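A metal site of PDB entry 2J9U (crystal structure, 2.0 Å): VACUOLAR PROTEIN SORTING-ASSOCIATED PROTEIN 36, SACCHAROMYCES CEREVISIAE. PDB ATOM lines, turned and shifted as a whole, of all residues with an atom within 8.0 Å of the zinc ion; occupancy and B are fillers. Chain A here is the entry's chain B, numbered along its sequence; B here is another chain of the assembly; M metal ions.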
ATOM      1  N   TRP A  18      11.138   9.971  14.529  1.00  0.00           N
ATOM      2  CA  TRP A  18      10.927   8.856  15.496  1.00  0.00           C
ATOM      3  C   TRP A  18      12.028   7.823  15.306  1.00  0.00           C
ATOM      4  O   TRP A  18      12.715   7.829  14.278  1.00  0.00           O
ATOM      5  CB  TRP A  18       9.557   8.182  15.357  1.00  0.00           C
ATOM      6  CG  TRP A  18       9.135   7.795  13.959  1.00  0.00           C
ATOM      7  CD1 TRP A  18       8.586   8.623  13.001  1.00  0.00           C
ATOM      8  CD2 TRP A  18       9.168   6.468  13.365  1.00  0.00           C
ATOM      9  NE1 TRP A  18       8.332   7.902  11.848  1.00  0.00           N
ATOM     10  CE2 TRP A  18       8.650   6.578  12.046  1.00  0.00           C
ATOM     11  CE3 TRP A  18       9.577   5.202  13.821  1.00  0.00           C
ATOM     12  CZ2 TRP A  18       8.563   5.483  11.171  1.00  0.00           C
ATOM     13  CZ3 TRP A  18       9.469   4.108  12.946  1.00  0.00           C
ATOM     14  CH2 TRP A  18       8.973   4.268  11.635  1.00  0.00           C
ATOM     15  N   VAL A  19      12.215   6.968  16.304  1.00  0.00           N
ATOM     16  CA  VAL A  19      13.173   5.871  16.155  1.00  0.00           C
ATOM     17  C   VAL A  19      12.481   4.500  16.159  1.00  0.00           C
ATOM     18  O   VAL A  19      11.675   4.212  17.037  1.00  0.00           O
ATOM     19  CB  VAL A  19      14.370   5.995  17.127  1.00  0.00           C
ATOM     20  CG1 VAL A  19      13.985   6.758  18.334  1.00  0.00           C
ATOM     21  CG2 VAL A  19      15.048   4.677  17.487  1.00  0.00           C
ATOM     22  N   CYS A  20      12.792   3.667  15.155  1.00  0.00           N
ATOM     23  CA  CYS A  20      12.163   2.370  15.036  1.00  0.00           C
ATOM     24  C   CYS A  20      12.499   1.531  16.294  1.00  0.00           C
ATOM     25  O   CYS A  20      13.681   1.317  16.600  1.00  0.00           O
ATOM     26  CB  CYS A  20      12.650   1.651  13.768  1.00  0.00           C
ATOM     27  SG  CYS A  20      11.970  -0.006  13.634  1.00  0.00           S
ATOM     28  N   PRO A  21      11.468   1.032  17.010  1.00  0.00           N
ATOM     29  CA  PRO A  21      11.715   0.204  18.218  1.00  0.00           C
ATOM     30  C   PRO A  21      12.235  -1.198  17.870  1.00  0.00           C
ATOM     31  O   PRO A  21      12.738  -1.899  18.723  1.00  0.00           O
ATOM     32  CB  PRO A  21      10.347   0.124  18.884  1.00  0.00           C
ATOM     33  CG  PRO A  21       9.328   0.248  17.752  1.00  0.00           C
ATOM     34  CD  PRO A  21      10.014   1.175  16.716  1.00  0.00           C
ATOM     35  N   ILE A  22      12.141  -1.589  16.594  1.00  0.00           N
ATOM     36  CA  ILE A  22      12.644  -2.904  16.182  1.00  0.00           C
ATOM     37  C   ILE A  22      14.148  -2.862  15.899  1.00  0.00           C
ATOM     38  O   ILE A  22      14.881  -3.630  16.506  1.00  0.00           O
ATOM     39  CB  ILE A  22      11.876  -3.443  14.950  1.00  0.00           C
ATOM     40  CG1 ILE A  22      10.346  -3.365  15.188  1.00  0.00           C
ATOM     41  CG2 ILE A  22      12.345  -4.865  14.562  1.00  0.00           C
ATOM     42  CD1 ILE A  22       9.800  -4.294  16.285  1.00  0.00           C
ATOM     43  N   CYS A  23      14.572  -1.963  14.972  1.00  0.00           N
ATOM     44  CA  CYS A  23      15.938  -1.916  14.477  1.00  0.00           C
ATOM     45  C   CYS A  23      16.753  -0.681  14.910  1.00  0.00           C
ATOM     46  O   CYS A  23      17.966  -0.646  14.715  1.00  0.00           O
ATOM     47  CB  CYS A  23      15.964  -2.051  12.952  1.00  0.00           C
ATOM     48  SG  CYS A  23      15.354  -0.609  12.017  1.00  0.00           S
ATOM     49  N   MET A  24      16.069   0.306  15.495  1.00  0.00           N
ATOM     50  CA  MET A  24      16.721   1.473  16.100  1.00  0.00           C
ATOM     51  C   MET A  24      17.171   2.559  15.116  1.00  0.00           C
ATOM     52  O   MET A  24      17.926   3.464  15.512  1.00  0.00           O
ATOM     53  CB  MET A  24      17.912   1.052  16.965  1.00  0.00           C
ATOM     54  CG  MET A  24      17.780   1.298  18.436  1.00  0.00           C
ATOM     55  SD  MET A  24      16.479   0.548  19.411  1.00  0.00           S
ATOM     56  CE  MET A  24      15.052   1.596  19.239  1.00  0.00           C
ATOM     57  N   VAL A  25      16.747   2.479  13.856  1.00  0.00           N
ATOM     58  CA  VAL A  25      17.096   3.530  12.893  1.00  0.00           C
ATOM     59  C   VAL A  25      16.110   4.705  12.968  1.00  0.00           C
ATOM     60  O   VAL A  25      14.933   4.521  13.209  1.00  0.00           O
ATOM     61  CB  VAL A  25      17.382   3.057  11.393  1.00  0.00           C
ATOM     62  CG1 VAL A  25      18.010   1.660  11.265  1.00  0.00           C
ATOM     63  CG2 VAL A  25      16.257   3.361  10.423  1.00  0.00           C
ATOM     64  N   SER A  26      16.649   5.911  12.770  1.00  0.00           N
ATOM     65  CA  SER A  26      15.826   7.139  12.773  1.00  0.00           C
ATOM     66  C   SER A  26      14.987   7.221  11.504  1.00  0.00           C
ATOM     67  O   SER A  26      15.520   7.058  10.403  1.00  0.00           O
ATOM     68  CB  SER A  26      16.734   8.364  12.807  1.00  0.00           C
ATOM     69  OG  SER A  26      17.074   8.679  14.136  1.00  0.00           O
ATOM     70  N   ASN A  27      13.694   7.498  11.665  1.00  0.00           N
ATOM     71  CA  ASN A  27      12.798   7.739  10.539  1.00  0.00           C
ATOM     72  C   ASN A  27      12.191   9.161  10.586  1.00  0.00           C
ATOM     73  O   ASN A  27      12.143   9.809  11.659  1.00  0.00           O
ATOM     74  CB  ASN A  27      11.686   6.702  10.547  1.00  0.00           C
ATOM     75  CG  ASN A  27      12.108   5.334   9.986  1.00  0.00           C
ATOM     76  OD1 ASN A  27      11.807   5.034   8.836  1.00  0.00           O
ATOM     77  ND2 ASN A  27      12.736   4.469  10.837  1.00  0.00           N
ATOM     78  N   ILE A  42       5.815   3.313   8.275  1.00  0.00           N
ATOM     79  CA  ILE A  42       6.599   2.101   8.140  1.00  0.00           C
ATOM     80  C   ILE A  42       8.081   2.478   8.183  1.00  0.00           C
ATOM     81  O   ILE A  42       8.485   3.441   7.564  1.00  0.00           O
ATOM     82  CB  ILE A  42       6.216   1.368   6.838  1.00  0.00           C
ATOM     83  CG1 ILE A  42       4.723   0.975   6.876  1.00  0.00           C
ATOM     84  CG2 ILE A  42       7.111   0.148   6.594  1.00  0.00           C
ATOM     85  CD1 ILE A  42       4.168   0.515   5.541  1.00  0.00           C
ATOM     86  N   CYS A  43       8.894   1.723   8.930  1.00  0.00           N
ATOM     87  CA  CYS A  43      10.330   1.930   8.939  1.00  0.00           C
ATOM     88  C   CYS A  43      10.993   1.681   7.552  1.00  0.00           C
ATOM     89  O   CYS A  43      10.785   0.630   6.944  1.00  0.00           O
ATOM     90  CB  CYS A  43      11.007   1.042   9.981  1.00  0.00           C
ATOM     91  SG  CYS A  43      12.819   1.131  10.098  1.00  0.00           S
ATOM     92  N   ILE A  44      11.795   2.639   7.105  1.00  0.00           N
ATOM     93  CA  ILE A  44      12.511   2.523   5.823  1.00  0.00           C
ATOM     94  C   ILE A  44      13.536   1.347   5.758  1.00  0.00           C
ATOM     95  O   ILE A  44      13.879   0.880   4.669  1.00  0.00           O
ATOM     96  CB  ILE A  44      13.195   3.868   5.450  1.00  0.00           C
ATOM     97  CG1 ILE A  44      13.615   3.863   3.971  1.00  0.00           C
ATOM     98  CG2 ILE A  44      14.378   4.159   6.335  1.00  0.00           C
ATOM     99  CD1 ILE A  44      12.727   4.734   3.089  1.00  0.00           C
ATOM    100  N   ASN A  45      13.994   0.871   6.922  1.00  0.00           N
ATOM    101  CA  ASN A  45      15.074  -0.101   6.979  1.00  0.00           C
ATOM    102  C   ASN A  45      14.549  -1.541   7.137  1.00  0.00           C
ATOM    103  O   ASN A  45      14.918  -2.416   6.345  1.00  0.00           O
ATOM    104  CB  ASN A  45      16.048   0.267   8.110  1.00  0.00           C
ATOM    105  CG  ASN A  45      17.207  -0.725   8.249  1.00  0.00           C
ATOM    106  OD1 ASN A  45      17.978  -0.919   7.300  1.00  0.00           O
ATOM    107  ND2 ASN A  45      17.351  -1.340   9.426  1.00  0.00           N
ATOM    108  N   CYS A  46      13.694  -1.793   8.134  1.00  0.00           N
ATOM    109  CA  CYS A  46      13.239  -3.189   8.401  1.00  0.00           C
ATOM    110  C   CYS A  46      11.826  -3.399   7.861  1.00  0.00           C
ATOM    111  O   CYS A  46      11.342  -4.529   7.766  1.00  0.00           O
ATOM    112  CB  CYS A  46      13.299  -3.498   9.915  1.00  0.00           C
ATOM    113  SG  CYS A  46      12.081  -2.548  10.899  1.00  0.00           S
ATOM    114  N   GLY A  47      11.182  -2.305   7.451  1.00  0.00           N
ATOM    115  CA  GLY A  47       9.833  -2.366   6.905  1.00  0.00           C
ATOM    116  C   GLY A  47       8.713  -2.782   7.868  1.00  0.00           C
ATOM    117  O   GLY A  47       7.635  -3.137   7.436  1.00  0.00           O
ATOM    118  N   VAL A  48       8.946  -2.714   9.177  1.00  0.00           N
ATOM    119  CA  VAL A  48       7.890  -3.000  10.164  1.00  0.00           C
ATOM    120  C   VAL A  48       7.087  -1.713  10.416  1.00  0.00           C
ATOM    121  O   VAL A  48       7.678  -0.670  10.645  1.00  0.00           O
ATOM    122  CB  VAL A  48       8.525  -3.546  11.472  1.00  0.00           C
ATOM    123  CG1 VAL A  48       7.449  -3.817  12.569  1.00  0.00           C
ATOM    124  CG2 VAL A  48       9.339  -4.816  11.150  1.00  0.00           C
ATOM    125  N   PRO A  49       5.716  -1.776  10.291  1.00  0.00           N
ATOM    126  CA  PRO A  49       4.877  -0.631  10.718  1.00  0.00           C
ATOM    127  C   PRO A  49       5.129  -0.247  12.185  1.00  0.00           C
ATOM    128  O   PRO A  49       5.106  -1.120  13.062  1.00  0.00           O
ATOM    129  CB  PRO A  49       3.461  -1.183  10.603  1.00  0.00           C
ATOM    130  CG  PRO A  49       3.583  -2.319   9.621  1.00  0.00           C
ATOM    131  CD  PRO A  49       4.913  -2.922   9.844  1.00  0.00           C
ATOM    132  N   ALA A  50       5.376   1.029  12.452  1.00  0.00           N
ATOM    133  CA  ALA A  50       5.691   1.477  13.817  1.00  0.00           C
ATOM    134  C   ALA A  50       4.556   1.234  14.821  1.00  0.00           C
ATOM    135  O   ALA A  50       3.420   1.681  14.626  1.00  0.00           O
ATOM    136  CB  ALA A  50       6.087   2.976  13.806  1.00  0.00           C
ATOM    137  N   ILE B  57      16.635  -9.595  14.295  1.00  0.00           N
ATOM    138  CA  ILE B  57      16.640  -8.260  13.658  1.00  0.00           C
ATOM    139  C   ILE B  57      17.360  -8.240  12.280  1.00  0.00           C
ATOM    140  O   ILE B  57      16.802  -7.735  11.275  1.00  0.00           O
ATOM    141  CB  ILE B  57      17.138  -7.144  14.615  1.00  0.00           C
ATOM    142  CG1 ILE B  57      16.230  -7.083  15.868  1.00  0.00           C
ATOM    143  CG2 ILE B  57      17.105  -5.742  13.885  1.00  0.00           C
ATOM    144  CD1 ILE B  57      16.843  -6.389  17.113  1.00  0.00           C
ATOM    145  N   ILE B  60      15.106  -9.936   9.587  1.00  0.00           N
ATOM    146  CA  ILE B  60      13.992  -9.184   9.038  1.00  0.00           C
ATOM    147  C   ILE B  60      14.475  -7.996   8.120  1.00  0.00           C
ATOM    148  O   ILE B  60      13.840  -7.729   7.094  1.00  0.00           O
ATOM    149  CB  ILE B  60      12.977  -8.757  10.105  1.00  0.00           C
ATOM    150  CG1 ILE B  60      11.641  -8.437   9.364  1.00  0.00           C
ATOM    151  CG2 ILE B  60      13.520  -7.531  10.847  1.00  0.00           C
ATOM    152  CD1 ILE B  60      10.508  -8.037  10.181  1.00  0.00           C
ATOM    153  N   VAL B  61      15.612  -7.366   8.460  1.00  0.00           N
ATOM    154  CA  VAL B  61      16.289  -6.361   7.601  1.00  0.00           C
ATOM    155  C   VAL B  61      16.721  -6.953   6.227  1.00  0.00           C
ATOM    156  O   VAL B  61      16.425  -6.389   5.140  1.00  0.00           O
ATOM    157  CB  VAL B  61      17.497  -5.647   8.338  1.00  0.00           C
ATOM    158  CG1 VAL B  61      18.293  -4.679   7.401  1.00  0.00           C
ATOM    159  CG2 VAL B  61      17.010  -4.897   9.625  1.00  0.00           C
ATOM    160  N   ASN B  64      13.506  -7.838   4.244  1.00  0.00           N
ATOM    161  CA  ASN B  64      12.978  -6.574   3.688  1.00  0.00           C
ATOM    162  C   ASN B  64      13.633  -6.068   2.379  1.00  0.00           C
ATOM    163  O   ASN B  64      12.969  -5.381   1.575  1.00  0.00           O
ATOM    164  CB  ASN B  64      13.015  -5.470   4.722  1.00  0.00           C
ATOM    165  CG  ASN B  64      12.132  -4.326   4.369  1.00  0.00           C
ATOM    166  OD1 ASN B  64      10.937  -4.511   4.090  1.00  0.00           O
ATOM    167  ND2 ASN B  64      12.689  -3.122   4.361  1.00  0.00           N
HETATM  168 ZN    ZN M   1      13.125  -0.626  11.655  1.00  0.00          ZN
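SG of Cys 23 sits close to ND2 of Asn 45 (3.4 Å). N of Val 48 sits close to SG of Cys 46 (3.6 Å). SG of Cys 43 lies close to N of Asn 45 (3.4 Å). SG of Cys 43 sits close to ND2 of Asn 27 (3.4 Å). O of Val 48 lies within hydrogen-bond range of N of Cys 43 (3.2 Å). SG of Cys 20 lies close to N of Ile 22, at 3.4 Å. The backbone NH of Cys 20 sits at hydrogen-bond distance from the backbone carbonyl oxygen of Val 25 (3.0 Å).
Four residues have an atom within 4 Å of the zinc ion: Cys 20, Cys 23, Cys 43 and Cys 46. The nearest printed residue that does not touch the zinc ion is Ile 22 (4.5 Å).
The side-chain sulfur (SG) of Cys 23 binds the zinc ion. SG of Cys 46 binds the zinc ion (2.3 Å). The side-chain sulfur (SG) of Cys 43 is bound to the zinc ion (2.4 Å). The zinc ion is bound by SG of Cys 20.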
